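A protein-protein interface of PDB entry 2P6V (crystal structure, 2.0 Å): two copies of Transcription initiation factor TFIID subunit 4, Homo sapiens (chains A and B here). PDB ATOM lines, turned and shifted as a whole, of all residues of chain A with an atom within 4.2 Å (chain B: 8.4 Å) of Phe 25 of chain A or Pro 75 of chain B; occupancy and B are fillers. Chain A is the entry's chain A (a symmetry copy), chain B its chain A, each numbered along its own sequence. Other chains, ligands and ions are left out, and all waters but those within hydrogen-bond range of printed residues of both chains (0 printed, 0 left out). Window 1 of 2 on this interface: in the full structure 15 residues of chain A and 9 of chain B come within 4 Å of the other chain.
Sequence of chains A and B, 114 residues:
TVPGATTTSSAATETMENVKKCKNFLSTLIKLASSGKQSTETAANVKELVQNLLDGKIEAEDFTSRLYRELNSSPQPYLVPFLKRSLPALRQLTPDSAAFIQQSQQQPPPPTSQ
O of Pro 75 of chain B lies within hydrogen-bond range of NE2 of Gln 76 of chain A, 3.0 Å away.
The backbone NH (N) of Ser 73 of chain B is in hydrogen-bond range of the backbone carbonyl oxygen (O) of Tyr 68 of chain B (2.8 Å).
The backbone NH (N) of Gln 76 of chain B lies within hydrogen-bond range of the side-chain hydroxyl (OH) of Tyr 68 of chain B (3.1 Å).
O of Asn 24 of chain A sits at hydrogen-bond distance from OG1 of Thr 28 of chain A (2.8 Å).
Among the printed residues, pairs that only touch across the chains: Leu 32 of chain A with Arg 69 of chain B, MLY 21 of chain A with Tyr 78 of chain B, Phe 25 of chain A with Pro 75 of chain B, Gln 76 of chain A with Pro 77 of chain B, Leu 32 of chain A with Ser 73 of chain B, Gln 76 of chain A with Gln 76 of chain B, Leu 29 of chain A with Pro 75 of chain B, Leu 79 of chain A with Pro 77 of chain B, Leu 32 of chain A with Pro 75 of chain B, Thr 28 of chain A with Pro 75 of chain B and Gln 76 of chain A with Ser 74 of chain B.
Of chain B, only Pro 75 comes within 4 Å of Phe 25 of chain A.
Of chain A, only Phe 25, Thr 28, Leu 29, Leu 32 and Gln 76 come within 4 Å of Pro 75 of chain B.
Of the printed residues of chain A, Ser 74 of chain B touches Gln 76.
Of the printed residues of chain B, Thr 28 of chain A touches Pro 75.
Printed residues of chain A within 4 Å of Pro 77 of chain B: Gln 76 (3.5 Å) and Leu 79 (3.8 Å).
Printed residues of chain B within 4 Å of Leu 29 of chain A: Pro 75 (3.7 Å).
The nearest residue of chain B that does not touch Phe 25 of chain A is Pro 77 of chain B (4.1 Å).
The nearest printed residue of chain A that does not touch Pro 75 of chain B is Leu 79 of chain A (5.4 Å).
Hydrophobic or aromatic side chains of chain B within 4 Å of the printed part of chain A: Pro 75, Pro 77 and Tyr 78.
Printed residues of chain A that touch a printed residue of chain B: MLY 21, Phe 25, Thr 28, Leu 29, Leu 32, Gln 76 and Leu 79.
Along chain A the printed residues that touch a printed residue of chain B span positions 21 to 79.
Among the printed residues, 12 pairs touch across the chains.
Gln 76 of chain A touches its own counterpart, Gln 76 of chain B.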
ATOM      1  N   MLY A  21     -29.569  -0.012  10.431  1.00  0.00           N
ATOM      2  CA  MLY A  21     -28.969  -0.669   9.267  1.00  0.00           C
ATOM      3  CB  MLY A  21     -27.805   0.156   8.742  1.00  0.00           C
ATOM      4  CG  MLY A  21     -28.425   1.340   7.983  1.00  0.00           C
ATOM      5  CD  MLY A  21     -27.292   2.128   7.318  1.00  0.00           C
ATOM      6  CE  MLY A  21     -26.626   3.097   8.267  1.00  0.00           C
ATOM      7  NZ  MLY A  21     -25.655   3.978   7.571  1.00  0.00           N
ATOM      8  CH1 MLY A  21     -25.252   4.994   8.563  1.00  0.00           C
ATOM      9  CH2 MLY A  21     -24.497   3.247   6.948  1.00  0.00           C
ATOM     10  C   MLY A  21     -28.519  -2.072   9.570  1.00  0.00           C
ATOM     11  O   MLY A  21     -28.637  -2.954   8.723  1.00  0.00           O
ATOM     12  N   CYS A  22     -27.972  -2.307  10.760  1.00  0.00           N
ATOM     13  CA  CYS A  22     -27.427  -3.625  11.050  1.00  0.00           C
ATOM     14  C   CYS A  22     -28.533  -4.630  11.291  1.00  0.00           C
ATOM     15  O   CYS A  22     -28.463  -5.788  10.899  1.00  0.00           O
ATOM     16  CB  CYS A  22     -26.509  -3.498  12.236  1.00  0.00           C
ATOM     17  SG  CYS A  22     -25.636  -4.989  12.701  1.00  0.00           S
ATOM     18  N   MLY A  23     -29.619  -4.183  11.907  1.00  0.00           N
ATOM     19  CA  MLY A  23     -30.798  -5.019  11.937  1.00  0.00           C
ATOM     20  CB  MLY A  23     -32.018  -4.292  12.531  1.00  0.00           C
ATOM     21  CG  MLY A  23     -32.049  -4.546  14.024  1.00  0.00           C
ATOM     22  CD  MLY A  23     -33.217  -3.820  14.694  1.00  0.00           C
ATOM     23  CE  MLY A  23     -34.536  -4.578  14.514  1.00  0.00           C
ATOM     24  NZ  MLY A  23     -35.524  -4.270  15.573  1.00  0.00           N
ATOM     25  CH1 MLY A  23     -36.261  -3.037  15.213  1.00  0.00           C
ATOM     26  CH2 MLY A  23     -36.417  -5.433  15.783  1.00  0.00           C
ATOM     27  C   MLY A  23     -31.326  -5.412  10.634  1.00  0.00           C
ATOM     28  O   MLY A  23     -31.711  -6.564  10.413  1.00  0.00           O
ATOM     29  N   ASN A  24     -31.381  -4.439   9.739  1.00  0.00           N
ATOM     30  CA  ASN A  24     -31.837  -4.737   8.385  1.00  0.00           C
ATOM     31  C   ASN A  24     -30.867  -5.699   7.654  1.00  0.00           C
ATOM     32  O   ASN A  24     -31.316  -6.621   6.928  1.00  0.00           O
ATOM     33  CB  ASN A  24     -32.066  -3.414   7.646  1.00  0.00           C
ATOM     34  CG  ASN A  24     -32.427  -3.606   6.178  1.00  0.00           C
ATOM     35  OD1 ASN A  24     -31.580  -3.419   5.298  1.00  0.00           O
ATOM     36  ND2 ASN A  24     -33.668  -4.012   5.911  1.00  0.00           N
ATOM     37  N   PHE A  25     -29.571  -5.519   7.897  1.00  0.00           N
ATOM     38  CA  PHE A  25     -28.567  -6.410   7.301  1.00  0.00           C
ATOM     39  C   PHE A  25     -28.798  -7.864   7.760  1.00  0.00           C
ATOM     40  O   PHE A  25     -28.878  -8.771   6.948  1.00  0.00           O
ATOM     41  CB  PHE A  25     -27.150  -5.936   7.737  1.00  0.00           C
ATOM     42  CG  PHE A  25     -26.073  -6.870   7.308  1.00  0.00           C
ATOM     43  CD1 PHE A  25     -25.725  -6.974   5.984  1.00  0.00           C
ATOM     44  CD2 PHE A  25     -25.441  -7.724   8.254  1.00  0.00           C
ATOM     45  CE1 PHE A  25     -24.762  -7.882   5.602  1.00  0.00           C
ATOM     46  CE2 PHE A  25     -24.513  -8.643   7.877  1.00  0.00           C
ATOM     47  CZ  PHE A  25     -24.163  -8.751   6.539  1.00  0.00           C
ATOM     48  N   LEU A  26     -28.835  -8.106   9.083  1.00  0.00           N
ATOM     49  CA  LEU A  26     -29.011  -9.442   9.579  1.00  0.00           C
ATOM     50  C   LEU A  26     -30.396 -10.026   9.243  1.00  0.00           C
ATOM     51  O   LEU A  26     -30.544 -11.221   8.875  1.00  0.00           O
ATOM     52  CB  LEU A  26     -28.755  -9.451  11.092  1.00  0.00           C
ATOM     53  CG  LEU A  26     -27.438  -8.961  11.573  1.00  0.00           C
ATOM     54  CD1 LEU A  26     -27.398  -8.936  13.081  1.00  0.00           C
ATOM     55  CD2 LEU A  26     -26.357  -9.964  11.003  1.00  0.00           C
ATOM     56  N   SER A  27     -31.409  -9.179   9.286  1.00  0.00           N
ATOM     57  CA  SER A  27     -32.733  -9.714   8.933  1.00  0.00           C
ATOM     58  C   SER A  27     -32.796 -10.016   7.451  1.00  0.00           C
ATOM     59  O   SER A  27     -33.364 -11.021   7.062  1.00  0.00           O
ATOM     60  CB  SER A  27     -33.868  -8.801   9.428  1.00  0.00           C
ATOM     61  OG  SER A  27     -34.172  -7.804   8.493  1.00  0.00           O
ATOM     62  N   THR A  28     -32.203  -9.205   6.576  1.00  0.00           N
ATOM     63  CA  THR A  28     -32.139  -9.634   5.184  1.00  0.00           C
ATOM     64  C   THR A  28     -31.423 -10.956   4.935  1.00  0.00           C
ATOM     65  O   THR A  28     -31.847 -11.726   4.109  1.00  0.00           O
ATOM     66  CB  THR A  28     -31.466  -8.523   4.337  1.00  0.00           C
ATOM     67  OG1 THR A  28     -32.274  -7.365   4.452  1.00  0.00           O
ATOM     68  CG2 THR A  28     -31.373  -8.898   2.920  1.00  0.00           C
ATOM     69  N   LEU A  29     -30.316 -11.206   5.643  1.00  0.00           N
ATOM     70  CA  LEU A  29     -29.646 -12.447   5.483  1.00  0.00           C
ATOM     71  C   LEU A  29     -30.561 -13.614   5.810  1.00  0.00           C
ATOM     72  O   LEU A  29     -30.612 -14.655   5.158  1.00  0.00           O
ATOM     73  CB  LEU A  29     -28.436 -12.471   6.423  1.00  0.00           C
ATOM     74  CG  LEU A  29     -27.085 -11.840   6.108  1.00  0.00           C
ATOM     75  CD1 LEU A  29     -26.282 -12.023   7.341  1.00  0.00           C
ATOM     76  CD2 LEU A  29     -26.533 -12.498   4.859  1.00  0.00           C
ATOM     77  N   LEU A  32     -33.242 -14.011   3.020  1.00  0.00           N
ATOM     78  CA  LEU A  32     -32.623 -14.641   1.849  1.00  0.00           C
ATOM     79  C   LEU A  32     -32.411 -16.117   2.121  1.00  0.00           C
ATOM     80  O   LEU A  32     -32.741 -16.939   1.291  1.00  0.00           O
ATOM     81  CB  LEU A  32     -31.261 -14.022   1.501  1.00  0.00           C
ATOM     82  CG  LEU A  32     -31.401 -12.555   1.048  1.00  0.00           C
ATOM     83  CD1 LEU A  32     -30.084 -11.849   0.898  1.00  0.00           C
ATOM     84  CD2 LEU A  32     -32.144 -12.504  -0.279  1.00  0.00           C
ATOM     85  N   GLN A  76     -16.394  -8.001   1.583  1.00  0.00           N
ATOM     86  CA  GLN A  76     -16.763  -6.596   1.733  1.00  0.00           C
ATOM     87  C   GLN A  76     -15.943  -5.878   2.774  1.00  0.00           C
ATOM     88  O   GLN A  76     -16.099  -6.047   4.018  1.00  0.00           O
ATOM     89  CB  GLN A  76     -18.231  -6.461   2.161  1.00  0.00           C
ATOM     90  CG  GLN A  76     -19.183  -7.115   1.225  1.00  0.00           C
ATOM     91  CD  GLN A  76     -20.662  -6.912   1.641  1.00  0.00           C
ATOM     92  OE1 GLN A  76     -21.025  -5.921   2.243  1.00  0.00           O
ATOM     93  NE2 GLN A  76     -21.458  -7.889   1.370  1.00  0.00           N
ATOM     94  N   LEU A  79     -17.553  -4.127   5.779  1.00  0.00           N
ATOM     95  CA  LEU A  79     -18.541  -4.902   6.533  1.00  0.00           C
ATOM     96  C   LEU A  79     -18.152  -5.165   7.998  1.00  0.00           C
ATOM     97  O   LEU A  79     -18.900  -4.977   8.941  1.00  0.00           O
ATOM     98  CB  LEU A  79     -18.838  -6.163   5.750  1.00  0.00           C
ATOM     99  CG  LEU A  79     -19.889  -7.125   6.374  1.00  0.00           C
ATOM    100  CD1 LEU A  79     -21.216  -6.414   6.743  1.00  0.00           C
ATOM    101  CD2 LEU A  79     -20.132  -8.383   5.602  1.00  0.00           C
ATOM    102  N   LEU A  83     -20.221  -3.742  11.374  1.00  0.00           N
ATOM    103  CA  LEU A  83     -20.734  -4.668  12.337  1.00  0.00           C
ATOM    104  C   LEU A  83     -20.161  -4.341  13.687  1.00  0.00           C
ATOM    105  O   LEU A  83     -20.891  -4.289  14.675  1.00  0.00           O
ATOM    106  CB  LEU A  83     -20.372  -6.099  11.956  1.00  0.00           C
ATOM    107  CG  LEU A  83     -21.191  -6.693  10.826  1.00  0.00           C
ATOM    108  CD1 LEU A  83     -20.729  -8.101  10.484  1.00  0.00           C
ATOM    109  CD2 LEU A  83     -22.730  -6.739  11.016  1.00  0.00           C
ATOM    110  N   THR B  64     -32.826  -3.057  -4.014  1.00  0.00           N
ATOM    111  CA  THR B  64     -31.696  -3.894  -3.516  1.00  0.00           C
ATOM    112  C   THR B  64     -32.189  -5.249  -3.001  1.00  0.00           C
ATOM    113  O   THR B  64     -31.583  -6.287  -3.279  1.00  0.00           O
ATOM    114  CB  THR B  64     -30.867  -3.213  -2.416  1.00  0.00           C
ATOM    115  OG1 THR B  64     -31.722  -2.847  -1.346  1.00  0.00           O
ATOM    116  CG2 THR B  64     -30.279  -1.930  -2.920  1.00  0.00           C
ATOM    117  N   SER B  65     -33.329  -5.238  -2.311  1.00  0.00           N
ATOM    118  CA  SER B  65     -33.939  -6.514  -1.845  1.00  0.00           C
ATOM    119  C   SER B  65     -34.202  -7.472  -2.961  1.00  0.00           C
ATOM    120  O   SER B  65     -33.955  -8.677  -2.877  1.00  0.00           O
ATOM    121  CB  SER B  65     -35.316  -6.305  -1.221  1.00  0.00           C
ATOM    122  OG  SER B  65     -35.168  -5.523  -0.058  1.00  0.00           O
ATOM    123  N   TYR B  68     -30.788  -8.744  -4.624  1.00  0.00           N
ATOM    124  CA  TYR B  68     -30.086  -9.792  -3.847  1.00  0.00           C
ATOM    125  C   TYR B  68     -30.731 -11.168  -4.089  1.00  0.00           C
ATOM    126  O   TYR B  68     -30.088 -12.198  -4.250  1.00  0.00           O
ATOM    127  CB  TYR B  68     -30.135  -9.508  -2.354  1.00  0.00           C
ATOM    128  CG  TYR B  68     -29.533  -8.228  -1.843  1.00  0.00           C
ATOM    129  CD1 TYR B  68     -28.384  -7.704  -2.395  1.00  0.00           C
ATOM    130  CD2 TYR B  68     -30.053  -7.604  -0.723  1.00  0.00           C
ATOM    131  CE1 TYR B  68     -27.828  -6.549  -1.921  1.00  0.00           C
ATOM    132  CE2 TYR B  68     -29.497  -6.434  -0.216  1.00  0.00           C
ATOM    133  CZ  TYR B  68     -28.388  -5.908  -0.877  1.00  0.00           C
ATOM    134  OH  TYR B  68     -27.784  -4.802  -0.358  1.00  0.00           O
ATOM    135  N   ARG B  69     -32.047 -11.174  -4.154  1.00  0.00           N
ATOM    136  CA  ARG B  69     -32.835 -12.380  -4.476  1.00  0.00           C
ATOM    137  C   ARG B  69     -32.550 -12.852  -5.897  1.00  0.00           C
ATOM    138  O   ARG B  69     -32.352 -14.036  -6.119  1.00  0.00           O
ATOM    139  CB  ARG B  69     -34.268 -12.180  -3.975  1.00  0.00           C
ATOM    140  CG  ARG B  69     -34.367 -11.793  -2.443  1.00  0.00           C
ATOM    141  CD  ARG B  69     -35.748 -11.267  -2.019  1.00  0.00           C
ATOM    142  NE  ARG B  69     -36.004 -11.288  -0.589  1.00  0.00           N
ATOM    143  CZ  ARG B  69     -36.190 -12.412   0.092  1.00  0.00           C
ATOM    144  NH1 ARG B  69     -36.122 -13.610  -0.505  1.00  0.00           N
ATOM    145  NH2 ARG B  69     -36.429 -12.312   1.389  1.00  0.00           N
ATOM    146  N   ASN B  72     -29.050 -13.981  -6.179  1.00  0.00           N
ATOM    147  CA  ASN B  72     -28.657 -14.744  -5.016  1.00  0.00           C
ATOM    148  C   ASN B  72     -27.361 -14.168  -4.510  1.00  0.00           C
ATOM    149  O   ASN B  72     -26.343 -14.845  -4.398  1.00  0.00           O
ATOM    150  CB  ASN B  72     -28.474 -16.227  -5.347  1.00  0.00           C
ATOM    151  CG  ASN B  72     -28.182 -17.029  -4.108  1.00  0.00           C
ATOM    152  OD1 ASN B  72     -28.902 -16.900  -3.116  1.00  0.00           O
ATOM    153  ND2 ASN B  72     -27.122 -17.840  -4.142  1.00  0.00           N
ATOM    154  N   SER B  73     -27.392 -12.879  -4.219  1.00  0.00           N
ATOM    155  CA  SER B  73     -26.231 -12.283  -3.591  1.00  0.00           C
ATOM    156  C   SER B  73     -26.517 -11.899  -2.151  1.00  0.00           C
ATOM    157  O   SER B  73     -27.654 -11.899  -1.687  1.00  0.00           O
ATOM    158  CB  SER B  73     -25.728 -11.045  -4.383  1.00  0.00           C
ATOM    159  OG  SER B  73     -26.747 -10.105  -4.649  1.00  0.00           O
ATOM    160  N   SER B  74     -25.414 -11.588  -1.468  1.00  0.00           N
ATOM    161  CA  SER B  74     -25.415 -11.129  -0.100  1.00  0.00           C
ATOM    162  C   SER B  74     -25.579  -9.585   0.083  1.00  0.00           C
ATOM    163  O   SER B  74     -25.121  -8.800  -0.762  1.00  0.00           O
ATOM    164  CB  SER B  74     -24.107 -11.630   0.511  1.00  0.00           C
ATOM    165  OG  SER B  74     -23.793 -10.985   1.738  1.00  0.00           O
ATOM    166  N   PRO B  75     -26.263  -9.150   1.166  1.00  0.00           N
ATOM    167  CA  PRO B  75     -26.492  -7.739   1.446  1.00  0.00           C
ATOM    168  C   PRO B  75     -25.225  -6.934   1.691  1.00  0.00           C
ATOM    169  O   PRO B  75     -24.255  -7.433   2.251  1.00  0.00           O
ATOM    170  CB  PRO B  75     -27.484  -7.723   2.638  1.00  0.00           C
ATOM    171  CG  PRO B  75     -27.508  -9.075   3.176  1.00  0.00           C
ATOM    172  CD  PRO B  75     -26.966 -10.027   2.141  1.00  0.00           C
ATOM    173  N   GLN B  76     -25.296  -5.692   1.221  1.00  0.00           N
ATOM    174  CA  GLN B  76     -24.333  -4.603   1.362  1.00  0.00           C
ATOM    175  C   GLN B  76     -24.890  -3.415   2.102  1.00  0.00           C
ATOM    176  O   GLN B  76     -25.722  -2.608   1.595  1.00  0.00           O
ATOM    177  CB  GLN B  76     -23.884  -4.091  -0.014  1.00  0.00           C
ATOM    178  CG  GLN B  76     -23.297  -5.150  -0.877  1.00  0.00           C
ATOM    179  CD  GLN B  76     -22.794  -4.600  -2.235  1.00  0.00           C
ATOM    180  OE1 GLN B  76     -22.385  -3.462  -2.351  1.00  0.00           O
ATOM    181  NE2 GLN B  76     -22.903  -5.403  -3.238  1.00  0.00           N
ATOM    182  N   PRO B  77     -24.466  -3.276   3.373  1.00  0.00           N
ATOM    183  CA  PRO B  77     -24.982  -2.251   4.260  1.00  0.00           C
ATOM    184  C   PRO B  77     -24.870  -0.771   3.795  1.00  0.00           C
ATOM    185  O   PRO B  77     -25.647   0.073   4.220  1.00  0.00           O
ATOM    186  CB  PRO B  77     -24.133  -2.425   5.525  1.00  0.00           C
ATOM    187  CG  PRO B  77     -23.472  -3.650   5.430  1.00  0.00           C
ATOM    188  CD  PRO B  77     -23.513  -4.167   4.049  1.00  0.00           C
ATOM    189  N   TYR B  78     -23.913  -0.489   2.933  1.00  0.00           N
ATOM    190  CA  TYR B  78     -23.745   0.909   2.500  1.00  0.00           C
ATOM    191  C   TYR B  78     -24.424   1.137   1.132  1.00  0.00           C
ATOM    192  O   TYR B  78     -24.445   2.269   0.640  1.00  0.00           O
ATOM    193  CB  TYR B  78     -22.265   1.341   2.491  1.00  0.00           C
ATOM    194  CG  TYR B  78     -21.655   1.391   3.884  1.00  0.00           C
ATOM    195  CD1 TYR B  78     -21.918   2.439   4.742  1.00  0.00           C
ATOM    196  CD2 TYR B  78     -20.912   0.327   4.373  1.00  0.00           C
ATOM    197  CE1 TYR B  78     -21.397   2.461   6.045  1.00  0.00           C
ATOM    198  CE2 TYR B  78     -20.409   0.334   5.668  1.00  0.00           C
ATOM    199  CZ  TYR B  78     -20.631   1.411   6.491  1.00  0.00           C
ATOM    200  OH  TYR B  78     -20.136   1.431   7.791  1.00  0.00           O
ATOM    201  N   LEU B  79     -24.986   0.088   0.550  1.00  0.00           N
ATOM    202  CA  LEU B  79     -25.534   0.185  -0.805  1.00  0.00           C
ATOM    203  C   LEU B  79     -26.802   1.050  -0.911  1.00  0.00           C
ATOM    204  O   LEU B  79     -26.960   1.923  -1.748  1.00  0.00           O
ATOM    205  CB  LEU B  79     -25.715  -1.220  -1.335  1.00  0.00           C
ATOM    206  CG  LEU B  79     -26.273  -1.339  -2.783  1.00  0.00           C
ATOM    207  CD1 LEU B  79     -25.479  -0.491  -3.809  1.00  0.00           C
ATOM    208  CD2 LEU B  79     -26.482  -2.739  -3.267  1.00  0.00           C
ATOM    209  N   VAL B  80     -27.770   0.813  -0.059  1.00  0.00           N
ATOM    210  CA  VAL B  80     -28.974   1.664  -0.081  1.00  0.00           C
ATOM    211  C   VAL B  80     -28.674   3.166   0.135  1.00  0.00           C
ATOM    212  O   VAL B  80     -29.104   4.011  -0.637  1.00  0.00           O
ATOM    213  CB  VAL B  80     -30.074   1.090   0.869  1.00  0.00           C
ATOM    214  CG1 VAL B  80     -31.169   2.100   1.106  1.00  0.00           C
ATOM    215  CG2 VAL B  80     -30.628  -0.180   0.279  1.00  0.00           C
